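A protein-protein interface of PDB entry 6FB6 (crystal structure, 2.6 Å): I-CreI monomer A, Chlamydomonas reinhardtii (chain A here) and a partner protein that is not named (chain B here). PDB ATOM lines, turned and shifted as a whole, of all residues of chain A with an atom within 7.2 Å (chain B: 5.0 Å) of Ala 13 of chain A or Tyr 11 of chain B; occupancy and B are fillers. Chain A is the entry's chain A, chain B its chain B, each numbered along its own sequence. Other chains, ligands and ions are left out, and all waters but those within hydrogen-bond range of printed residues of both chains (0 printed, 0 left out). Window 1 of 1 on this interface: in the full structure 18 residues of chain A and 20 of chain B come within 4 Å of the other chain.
Among the printed residues, merely in contact across the chains: Leu 10 of chain A with Tyr 11 of chain B (3.3 Å), Phe 15 of chain A with Gly 14 of chain B (3.3 Å), Tyr 11 of chain A with Leu 10 of chain B (3.3 Å), Lys 95 of chain A with Tyr 11 of chain B (3.4 Å), Gly 14 of chain A with Tyr 11 of chain B (3.4 Å), Tyr 11 of chain A with Gly 14 of chain B (3.5 Å), Gly 14 of chain A with Gly 14 of chain B (3.5 Å), Leu 96 of chain A with Phe 53 of chain B (3.5 Å), Phe 93 of chain A with Tyr 11 of chain B (3.6 Å), Leu 10 of chain A with Glu 7 of chain B (3.6 Å), Leu 96 of chain A with Phe 15 of chain B (3.6 Å), Ser 18 of chain A with Phe 15 of chain B (3.6 Å), Ser 18 of chain A with Gly 14 of chain B (3.7 Å), Glu 7 of chain A with Leu 10 of chain B (3.7 Å), Phe 15 of chain A with Phe 15 of chain B (3.8 Å), Asp 17 of chain A with Phe 15 of chain B (3.8 Å), Tyr 11 of chain A with Ala 13 of chain B (3.8 Å), Ala 13 of chain A with Tyr 11 of chain B (3.8 Å) and Leu 10 of chain A with Leu 10 of chain B (3.9 Å).
The side-chain hydroxyl of Ser 18 of chain A lies within hydrogen-bond range of the backbone carbonyl oxygen of Gly 14 of chain A (3.2 Å).
The backbone carbonyl oxygen of Phe 15 of chain A lies within hydrogen-bond range of the side-chain hydroxyl of Ser 18 of chain A (2.7 Å).
The backbone NH (N) of Lys 95 of chain A sits at hydrogen-bond distance from the side-chain carboxylate (OD2) of Asp 17 of chain A.
N of Leu 96 of chain A sits at hydrogen-bond distance from OD2 of Asp 17 of chain A (3.2 Å).
The backbone NH (N) of Lys 97 of chain A sits at hydrogen-bond distance from the side-chain carboxylate (OD1) of Asp 17 of chain A (3.1 Å).
N of Phe 15 of chain B sits close to O of Gly 14 of chain A, 3.5 Å away.
The side-chain carboxylate (OD2) of Asp 17 of chain A lies within hydrogen-bond range of the side-chain hydroxyl (OH) of Tyr 11 of chain B.
Of the printed residues of chain B, Leu 10 of chain A touches Glu 7, Leu 10 and Tyr 11.
Of chain B, only Tyr 11 comes within 4 Å of Ala 13 of chain A.
Of the printed residues of chain A, Phe 53 of chain B touches Leu 96 (3.5 Å).
The nearest printed residue of chain B that does not touch Ala 13 of chain A is Phe 15 of chain B (5.7 Å).
The nearest printed residue of chain B that does not touch Tyr 11 of chain A is Tyr 11 of chain B (4.6 Å).
Of the 20 printed residues of chain A, 11 touch a printed residue of chain B.
Printed residues of chain A that touch a printed residue of chain B: Glu 7, Leu 10, Tyr 11, Ala 13, Gly 14, Phe 15, Asp 17, Ser 18, Phe 93, Lys 95 and Leu 96.
Hydrophobic or aromatic side chains of chain A that line the printed part of chain B: Leu 10, Tyr 11, Phe 15 and Leu 96.
Hydrophobic or aromatic side chains of chain B within 4 Å of the printed part of chain A: Leu 10, Tyr 11, Ala 13, Phe 15 and Phe 53.
Among the printed residues, no Asp or Glu carboxylate lies within 4 Å of a Lys or Arg side-chain nitrogen of the other chain.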
ATOM      1  N   GLU A   7       9.858   8.477  -1.541  1.00  0.00           N
ATOM      2  CA  GLU A   7      10.074   7.102  -1.105  1.00  0.00           C
ATOM      3  C   GLU A   7       9.424   6.854   0.252  1.00  0.00           C
ATOM      4  O   GLU A   7       8.964   5.748   0.540  1.00  0.00           O
ATOM      5  CB  GLU A   7      11.566   6.773  -1.046  1.00  0.00           C
ATOM      6  CG  GLU A   7      12.231   6.687  -2.408  1.00  0.00           C
ATOM      7  CD  GLU A   7      13.660   6.197  -2.325  1.00  0.00           C
ATOM      8  OE1 GLU A   7      14.141   5.953  -1.199  1.00  0.00           O
ATOM      9  OE2 GLU A   7      14.305   6.054  -3.385  1.00  0.00           O
ATOM     10  N   PHE A   8       9.385   7.891   1.082  1.00  0.00           N
ATOM     11  CA  PHE A   8       8.750   7.802   2.390  1.00  0.00           C
ATOM     12  C   PHE A   8       7.235   7.691   2.255  1.00  0.00           C
ATOM     13  O   PHE A   8       6.592   6.941   2.987  1.00  0.00           O
ATOM     14  CB  PHE A   8       9.129   9.011   3.245  1.00  0.00           C
ATOM     15  CG  PHE A   8       8.187   9.273   4.384  1.00  0.00           C
ATOM     16  CD1 PHE A   8       8.202   8.469   5.510  1.00  0.00           C
ATOM     17  CD2 PHE A   8       7.297  10.337   4.337  1.00  0.00           C
ATOM     18  CE1 PHE A   8       7.344   8.711   6.559  1.00  0.00           C
ATOM     19  CE2 PHE A   8       6.434  10.583   5.388  1.00  0.00           C
ATOM     20  CZ  PHE A   8       6.459   9.769   6.499  1.00  0.00           C
ATOM     21  N   LEU A   9       6.673   8.443   1.313  1.00  0.00           N
ATOM     22  CA  LEU A   9       5.238   8.416   1.056  1.00  0.00           C
ATOM     23  C   LEU A   9       4.798   7.071   0.483  1.00  0.00           C
ATOM     24  O   LEU A   9       3.721   6.577   0.807  1.00  0.00           O
ATOM     25  CB  LEU A   9       4.840   9.550   0.110  1.00  0.00           C
ATOM     26  CG  LEU A   9       4.937  10.960   0.688  1.00  0.00           C
ATOM     27  CD1 LEU A   9       4.751  12.005  -0.398  1.00  0.00           C
ATOM     28  CD2 LEU A   9       3.904  11.140   1.783  1.00  0.00           C
ATOM     29  N   LEU A  10       5.636   6.486  -0.367  1.00  0.00           N
ATOM     30  CA  LEU A  10       5.338   5.186  -0.957  1.00  0.00           C
ATOM     31  C   LEU A  10       5.297   4.079   0.089  1.00  0.00           C
ATOM     32  O   LEU A  10       4.399   3.237   0.077  1.00  0.00           O
ATOM     33  CB  LEU A  10       6.344   4.847  -2.058  1.00  0.00           C
ATOM     34  CG  LEU A  10       5.944   5.309  -3.457  1.00  0.00           C
ATOM     35  CD1 LEU A  10       7.144   5.310  -4.381  1.00  0.00           C
ATOM     36  CD2 LEU A  10       4.849   4.409  -4.005  1.00  0.00           C
ATOM     37  N   TYR A  11       6.268   4.077   0.995  1.00  0.00           N
ATOM     38  CA  TYR A  11       6.274   3.083   2.059  1.00  0.00           C
ATOM     39  C   TYR A  11       5.094   3.303   3.002  1.00  0.00           C
ATOM     40  O   TYR A  11       4.430   2.352   3.414  1.00  0.00           O
ATOM     41  CB  TYR A  11       7.590   3.116   2.839  1.00  0.00           C
ATOM     42  CG  TYR A  11       7.591   2.192   4.038  1.00  0.00           C
ATOM     43  CD1 TYR A  11       7.991   0.868   3.917  1.00  0.00           C
ATOM     44  CD2 TYR A  11       7.176   2.639   5.288  1.00  0.00           C
ATOM     45  CE1 TYR A  11       7.983   0.017   5.011  1.00  0.00           C
ATOM     46  CE2 TYR A  11       7.160   1.797   6.383  1.00  0.00           C
ATOM     47  CZ  TYR A  11       7.566   0.488   6.241  1.00  0.00           C
ATOM     48  OH  TYR A  11       7.552  -0.348   7.336  1.00  0.00           O
ATOM     49  N   LEU A  12       4.840   4.565   3.338  1.00  0.00           N
ATOM     50  CA  LEU A  12       3.789   4.908   4.290  1.00  0.00           C
ATOM     51  C   LEU A  12       2.407   4.558   3.758  1.00  0.00           C
ATOM     52  O   LEU A  12       1.564   4.058   4.500  1.00  0.00           O
ATOM     53  CB  LEU A  12       3.852   6.390   4.654  1.00  0.00           C
ATOM     54  CG  LEU A  12       2.944   6.827   5.801  1.00  0.00           C
ATOM     55  CD1 LEU A  12       3.222   5.981   7.031  1.00  0.00           C
ATOM     56  CD2 LEU A  12       3.146   8.299   6.109  1.00  0.00           C
ATOM     57  N   ALA A  13       2.180   4.819   2.473  1.00  0.00           N
ATOM     58  CA  ALA A  13       0.908   4.492   1.840  1.00  0.00           C
ATOM     59  C   ALA A  13       0.608   3.001   1.948  1.00  0.00           C
ATOM     60  O   ALA A  13      -0.545   2.602   2.098  1.00  0.00           O
ATOM     61  CB  ALA A  13       0.913   4.925   0.387  1.00  0.00           C
ATOM     62  N   GLY A  14       1.653   2.184   1.868  1.00  0.00           N
ATOM     63  CA  GLY A  14       1.504   0.748   1.994  1.00  0.00           C
ATOM     64  C   GLY A  14       1.102   0.362   3.402  1.00  0.00           C
ATOM     65  O   GLY A  14       0.196  -0.448   3.604  1.00  0.00           O
ATOM     66  N   PHE A  15       1.776   0.956   4.380  1.00  0.00           N
ATOM     67  CA  PHE A  15       1.489   0.691   5.782  1.00  0.00           C
ATOM     68  C   PHE A  15       0.123   1.236   6.190  1.00  0.00           C
ATOM     69  O   PHE A  15      -0.536   0.692   7.073  1.00  0.00           O
ATOM     70  CB  PHE A  15       2.573   1.303   6.667  1.00  0.00           C
ATOM     71  CG  PHE A  15       2.653   0.686   8.028  1.00  0.00           C
ATOM     72  CD1 PHE A  15       3.388  -0.469   8.232  1.00  0.00           C
ATOM     73  CD2 PHE A  15       1.990   1.253   9.103  1.00  0.00           C
ATOM     74  CE1 PHE A  15       3.463  -1.046   9.482  1.00  0.00           C
ATOM     75  CE2 PHE A  15       2.061   0.679  10.362  1.00  0.00           C
ATOM     76  CZ  PHE A  15       2.798  -0.470  10.552  1.00  0.00           C
ATOM     77  N   VAL A  16      -0.293   2.320   5.544  1.00  0.00           N
ATOM     78  CA  VAL A  16      -1.583   2.933   5.827  1.00  0.00           C
ATOM     79  C   VAL A  16      -2.719   2.076   5.279  1.00  0.00           C
ATOM     80  O   VAL A  16      -3.744   1.895   5.938  1.00  0.00           O
ATOM     81  CB  VAL A  16      -1.666   4.369   5.265  1.00  0.00           C
ATOM     82  CG1 VAL A  16      -3.102   4.875   5.266  1.00  0.00           C
ATOM     83  CG2 VAL A  16      -0.784   5.293   6.075  1.00  0.00           C
ATOM     84  N   ASP A  17      -2.530   1.537   4.079  1.00  0.00           N
ATOM     85  CA  ASP A  17      -3.528   0.662   3.479  1.00  0.00           C
ATOM     86  C   ASP A  17      -3.677  -0.634   4.267  1.00  0.00           C
ATOM     87  O   ASP A  17      -4.712  -1.302   4.191  1.00  0.00           O
ATOM     88  CB  ASP A  17      -3.171   0.354   2.026  1.00  0.00           C
ATOM     89  CG  ASP A  17      -3.517   1.490   1.095  1.00  0.00           C
ATOM     90  OD1 ASP A  17      -4.377   2.314   1.465  1.00  0.00           O
ATOM     91  OD2 ASP A  17      -2.933   1.556  -0.008  1.00  0.00           O
ATOM     92  N   SER A  18      -2.646  -0.980   5.031  1.00  0.00           N
ATOM     93  CA  SER A  18      -2.655  -2.210   5.809  1.00  0.00           C
ATOM     94  C   SER A  18      -3.176  -1.996   7.230  1.00  0.00           C
ATOM     95  O   SER A  18      -4.238  -2.509   7.586  1.00  0.00           O
ATOM     96  CB  SER A  18      -1.259  -2.832   5.845  1.00  0.00           C
ATOM     97  OG  SER A  18      -0.313  -1.944   6.417  1.00  0.00           O
ATOM     98  N   LEU A  90      -0.011  12.235   0.185  1.00  0.00           N
ATOM     99  CA  LEU A  90      -0.110  10.798   0.409  1.00  0.00           C
ATOM    100  C   LEU A  90      -1.125  10.127  -0.515  1.00  0.00           C
ATOM    101  O   LEU A  90      -0.970   8.957  -0.875  1.00  0.00           O
ATOM    102  CB  LEU A  90      -0.461  10.514   1.869  1.00  0.00           C
ATOM    103  CG  LEU A  90      -0.535   9.043   2.276  1.00  0.00           C
ATOM    104  CD1 LEU A  90       0.814   8.381   2.074  1.00  0.00           C
ATOM    105  CD2 LEU A  90      -0.995   8.904   3.715  1.00  0.00           C
ATOM    106  N   GLN A  91      -2.156  10.876  -0.897  1.00  0.00           N
ATOM    107  CA  GLN A  91      -3.242  10.357  -1.732  1.00  0.00           C
ATOM    108  C   GLN A  91      -2.840   9.603  -3.014  1.00  0.00           C
ATOM    109  O   GLN A  91      -3.391   8.536  -3.283  1.00  0.00           O
ATOM    110  CB  GLN A  91      -4.247  11.470  -2.055  1.00  0.00           C
ATOM    111  CG  GLN A  91      -5.415  11.041  -2.929  1.00  0.00           C
ATOM    112  CD  GLN A  91      -5.143  11.235  -4.407  1.00  0.00           C
ATOM    113  OE1 GLN A  91      -4.211  11.940  -4.791  1.00  0.00           O
ATOM    114  NE2 GLN A  91      -5.956  10.603  -5.246  1.00  0.00           N
ATOM    115  N   PRO A  92      -1.901  10.149  -3.814  1.00  0.00           N
ATOM    116  CA  PRO A  92      -1.608   9.484  -5.092  1.00  0.00           C
ATOM    117  C   PRO A  92      -1.012   8.083  -4.954  1.00  0.00           C
ATOM    118  O   PRO A  92      -1.016   7.323  -5.922  1.00  0.00           O
ATOM    119  CB  PRO A  92      -0.582  10.417  -5.742  1.00  0.00           C
ATOM    120  CG  PRO A  92      -0.814  11.731  -5.113  1.00  0.00           C
ATOM    121  CD  PRO A  92      -1.175  11.426  -3.699  1.00  0.00           C
ATOM    122  N   PHE A  93      -0.511   7.748  -3.771  1.00  0.00           N
ATOM    123  CA  PHE A  93       0.130   6.456  -3.566  1.00  0.00           C
ATOM    124  C   PHE A  93      -0.785   5.459  -2.860  1.00  0.00           C
ATOM    125  O   PHE A  93      -0.472   4.273  -2.783  1.00  0.00           O
ATOM    126  CB  PHE A  93       1.436   6.627  -2.788  1.00  0.00           C
ATOM    127  CG  PHE A  93       2.376   7.621  -3.404  1.00  0.00           C
ATOM    128  CD1 PHE A  93       2.975   7.359  -4.625  1.00  0.00           C
ATOM    129  CD2 PHE A  93       2.657   8.821  -2.770  1.00  0.00           C
ATOM    130  CE1 PHE A  93       3.837   8.271  -5.203  1.00  0.00           C
ATOM    131  CE2 PHE A  93       3.522   9.739  -3.343  1.00  0.00           C
ATOM    132  CZ  PHE A  93       4.112   9.462  -4.562  1.00  0.00           C
ATOM    133  N   LEU A  94      -1.911   5.943  -2.346  1.00  0.00           N
ATOM    134  CA  LEU A  94      -2.873   5.073  -1.684  1.00  0.00           C
ATOM    135  C   LEU A  94      -3.599   4.205  -2.700  1.00  0.00           C
ATOM    136  O   LEU A  94      -3.895   4.647  -3.806  1.00  0.00           O
ATOM    137  CB  LEU A  94      -3.876   5.891  -0.874  1.00  0.00           C
ATOM    138  CG  LEU A  94      -3.388   6.459   0.459  1.00  0.00           C
ATOM    139  CD1 LEU A  94      -4.481   7.291   1.106  1.00  0.00           C
ATOM    140  CD2 LEU A  94      -2.946   5.339   1.387  1.00  0.00           C
ATOM    141  N   LYS A  95      -3.885   2.967  -2.318  1.00  0.00           N
ATOM    142  CA  LYS A  95      -4.545   2.039  -3.223  1.00  0.00           C
ATOM    143  C   LYS A  95      -5.836   1.492  -2.636  1.00  0.00           C
ATOM    144  O   LYS A  95      -6.790   1.237  -3.366  1.00  0.00           O
ATOM    145  CB  LYS A  95      -3.605   0.891  -3.595  1.00  0.00           C
ATOM    146  CG  LYS A  95      -2.312   1.352  -4.233  1.00  0.00           C
ATOM    147  CD  LYS A  95      -1.512   0.186  -4.773  1.00  0.00           C
ATOM    148  CE  LYS A  95      -0.234   0.670  -5.432  1.00  0.00           C
ATOM    149  NZ  LYS A  95       0.471  -0.433  -6.133  1.00  0.00           N
ATOM    150  N   LEU A  96      -5.869   1.316  -1.319  1.00  0.00           N
ATOM    151  CA  LEU A  96      -7.055   0.775  -0.662  1.00  0.00           C
ATOM    152  C   LEU A  96      -7.864   1.865   0.025  1.00  0.00           C
ATOM    153  O   LEU A  96      -9.059   1.702   0.264  1.00  0.00           O
ATOM    154  CB  LEU A  96      -6.674  -0.296   0.360  1.00  0.00           C
ATOM    155  CG  LEU A  96      -6.050  -1.586  -0.161  1.00  0.00           C
ATOM    156  CD1 LEU A  96      -5.937  -2.594   0.969  1.00  0.00           C
ATOM    157  CD2 LEU A  96      -6.870  -2.148  -1.308  1.00  0.00           C
ATOM    158  N   LYS A  97      -7.206   2.973   0.347  1.00  0.00           N
ATOM    159  CA  LYS A  97      -7.862   4.058   1.063  1.00  0.00           C
ATOM    160  C   LYS A  97      -7.758   5.380   0.308  1.00  0.00           C
ATOM    161  O   LYS A  97      -7.899   6.455   0.894  1.00  0.00           O
ATOM    162  CB  LYS A  97      -7.285   4.190   2.475  1.00  0.00           C
ATOM    163  CG  LYS A  97      -7.431   2.926   3.314  1.00  0.00           C
ATOM    164  CD  LYS A  97      -6.815   3.088   4.697  1.00  0.00           C
ATOM    165  CE  LYS A  97      -6.912   1.799   5.501  1.00  0.00           C
ATOM    166  NZ  LYS A  97      -8.316   1.322   5.639  1.00  0.00           N
ATOM    167  N   GLU B   7       9.453   1.412  -6.902  1.00  0.00           N
ATOM    168  CA  GLU B   7       8.269   2.035  -6.313  1.00  0.00           C
ATOM    169  C   GLU B   7       7.245   0.980  -5.913  1.00  0.00           C
ATOM    170  O   GLU B   7       6.467   1.172  -4.976  1.00  0.00           O
ATOM    171  CB  GLU B   7       7.643   3.043  -7.277  1.00  0.00           C
ATOM    172  CG  GLU B   7       8.519   4.255  -7.549  1.00  0.00           C
ATOM    173  CD  GLU B   7       7.774   5.369  -8.262  1.00  0.00           C
ATOM    174  OE1 GLU B   7       6.620   5.142  -8.682  1.00  0.00           O
ATOM    175  OE2 GLU B   7       8.340   6.473  -8.398  1.00  0.00           O
ATOM    176  N   PHE B   8       7.255  -0.139  -6.628  1.00  0.00           N
ATOM    177  CA  PHE B   8       6.404  -1.267  -6.289  1.00  0.00           C
ATOM    178  C   PHE B   8       6.871  -1.926  -4.992  1.00  0.00           C
ATOM    179  O   PHE B   8       6.060  -2.233  -4.118  1.00  0.00           O
ATOM    180  CB  PHE B   8       6.390  -2.278  -7.435  1.00  0.00           C
ATOM    181  CG  PHE B   8       5.877  -3.631  -7.044  1.00  0.00           C
ATOM    182  CD1 PHE B   8       4.524  -3.837  -6.827  1.00  0.00           C
ATOM    183  CD2 PHE B   8       6.746  -4.702  -6.901  1.00  0.00           C
ATOM    184  CE1 PHE B   8       4.046  -5.081  -6.467  1.00  0.00           C
ATOM    185  CE2 PHE B   8       6.272  -5.950  -6.542  1.00  0.00           C
ATOM    186  CZ  PHE B   8       4.918  -6.138  -6.326  1.00  0.00           C
ATOM    187  N   LEU B   9       8.178  -2.136  -4.869  1.00  0.00           N
ATOM    188  CA  LEU B   9       8.741  -2.756  -3.674  1.00  0.00           C
ATOM    189  C   LEU B   9       8.583  -1.868  -2.441  1.00  0.00           C
ATOM    190  O   LEU B   9       8.419  -2.366  -1.327  1.00  0.00           O
ATOM    191  CB  LEU B   9      10.214  -3.104  -3.885  1.00  0.00           C
ATOM    192  CG  LEU B   9      10.524  -4.194  -4.907  1.00  0.00           C
ATOM    193  CD1 LEU B   9      12.020  -4.268  -5.149  1.00  0.00           C
ATOM    194  CD2 LEU B   9       9.995  -5.531  -4.425  1.00  0.00           C
ATOM    195  N   LEU B  10       8.636  -0.556  -2.641  1.00  0.00           N
ATOM    196  CA  LEU B  10       8.479   0.389  -1.541  1.00  0.00           C
ATOM    197  C   LEU B  10       7.074   0.351  -0.940  1.00  0.00           C
ATOM    198  O   LEU B  10       6.917   0.328   0.280  1.00  0.00           O
ATOM    199  CB  LEU B  10       8.829   1.807  -1.994  1.00  0.00           C
ATOM    200  CG  LEU B  10      10.313   2.169  -1.967  1.00  0.00           C
ATOM    201  CD1 LEU B  10      10.588   3.354  -2.878  1.00  0.00           C
ATOM    202  CD2 LEU B  10      10.743   2.482  -0.544  1.00  0.00           C
ATOM    203  N   TYR B  11       6.058   0.344  -1.797  1.00  0.00           N
ATOM    204  CA  TYR B  11       4.681   0.285  -1.326  1.00  0.00           C
ATOM    205  C   TYR B  11       4.419  -1.060  -0.664  1.00  0.00           C
ATOM    206  O   TYR B  11       3.846  -1.129   0.425  1.00  0.00           O
ATOM    207  CB  TYR B  11       3.702   0.502  -2.486  1.00  0.00           C
ATOM    208  CG  TYR B  11       2.252   0.248  -2.124  1.00  0.00           C
ATOM    209  CD1 TYR B  11       1.430   1.280  -1.693  1.00  0.00           C
ATOM    210  CD2 TYR B  11       1.702  -1.028  -2.217  1.00  0.00           C
ATOM    211  CE1 TYR B  11       0.103   1.048  -1.360  1.00  0.00           C
ATOM    212  CE2 TYR B  11       0.384  -1.268  -1.882  1.00  0.00           C
ATOM    213  CZ  TYR B  11      -0.412  -0.230  -1.457  1.00  0.00           C
ATOM    214  OH  TYR B  11      -1.728  -0.477  -1.131  1.00  0.00           O
ATOM    215  N   LEU B  12       4.844  -2.124  -1.339  1.00  0.00           N
ATOM    216  CA  LEU B  12       4.597  -3.483  -0.880  1.00  0.00           C
ATOM    217  C   LEU B  12       5.230  -3.746   0.480  1.00  0.00           C
ATOM    218  O   LEU B  12       4.662  -4.461   1.303  1.00  0.00           O
ATOM    219  CB  LEU B  12       5.120  -4.492  -1.902  1.00  0.00           C
ATOM    220  CG  LEU B  12       4.810  -5.957  -1.604  1.00  0.00           C
ATOM    221  CD1 LEU B  12       3.308  -6.168  -1.528  1.00  0.00           C
ATOM    222  CD2 LEU B  12       5.427  -6.851  -2.659  1.00  0.00           C
ATOM    223  N   ALA B  13       6.402  -3.163   0.711  1.00  0.00           N
ATOM    224  CA  ALA B  13       7.098  -3.320   1.982  1.00  0.00           C
ATOM    225  C   ALA B  13       6.239  -2.818   3.134  1.00  0.00           C
ATOM    226  O   ALA B  13       6.105  -3.492   4.158  1.00  0.00           O
ATOM    227  CB  ALA B  13       8.427  -2.588   1.956  1.00  0.00           C
ATOM    228  N   GLY B  14       5.661  -1.634   2.960  1.00  0.00           N
ATOM    229  CA  GLY B  14       4.806  -1.047   3.975  1.00  0.00           C
ATOM    230  C   GLY B  14       3.594  -1.915   4.247  1.00  0.00           C
ATOM    231  O   GLY B  14       3.214  -2.131   5.396  1.00  0.00           O
ATOM    232  N   PHE B  15       2.998  -2.426   3.176  1.00  0.00           N
ATOM    233  CA  PHE B  15       1.810  -3.259   3.285  1.00  0.00           C
ATOM    234  C   PHE B  15       2.133  -4.600   3.936  1.00  0.00           C
ATOM    235  O   PHE B  15       1.355  -5.115   4.743  1.00  0.00           O
ATOM    236  CB  PHE B  15       1.196  -3.482   1.907  1.00  0.00           C
ATOM    237  CG  PHE B  15      -0.219  -3.970   1.952  1.00  0.00           C
ATOM    238  CD1 PHE B  15      -0.494  -5.324   2.010  1.00  0.00           C
ATOM    239  CD2 PHE B  15      -1.273  -3.077   1.936  1.00  0.00           C
ATOM    240  CE1 PHE B  15      -1.795  -5.776   2.052  1.00  0.00           C
ATOM    241  CE2 PHE B  15      -2.577  -3.525   1.978  1.00  0.00           C
ATOM    242  CZ  PHE B  15      -2.836  -4.877   2.037  1.00  0.00           C
ATOM    243  N   PHE B  53      -7.255  -7.262  -4.830  1.00  0.00           N
ATOM    244  CA  PHE B  53      -5.971  -6.707  -4.431  1.00  0.00           C
ATOM    245  C   PHE B  53      -4.904  -7.797  -4.345  1.00  0.00           C
ATOM    246  O   PHE B  53      -3.769  -7.595  -4.774  1.00  0.00           O
ATOM    247  CB  PHE B  53      -6.107  -5.980  -3.092  1.00  0.00           C
ATOM    248  CG  PHE B  53      -4.851  -5.297  -2.647  1.00  0.00           C
ATOM    249  CD1 PHE B  53      -4.525  -4.042  -3.126  1.00  0.00           C
ATOM    250  CD2 PHE B  53      -3.996  -5.907  -1.747  1.00  0.00           C
ATOM    251  CE1 PHE B  53      -3.370  -3.408  -2.717  1.00  0.00           C
ATOM    252  CE2 PHE B  53      -2.840  -5.278  -1.338  1.00  0.00           C
ATOM    253  CZ  PHE B  53      -2.528  -4.026  -1.822  1.00  0.00           C
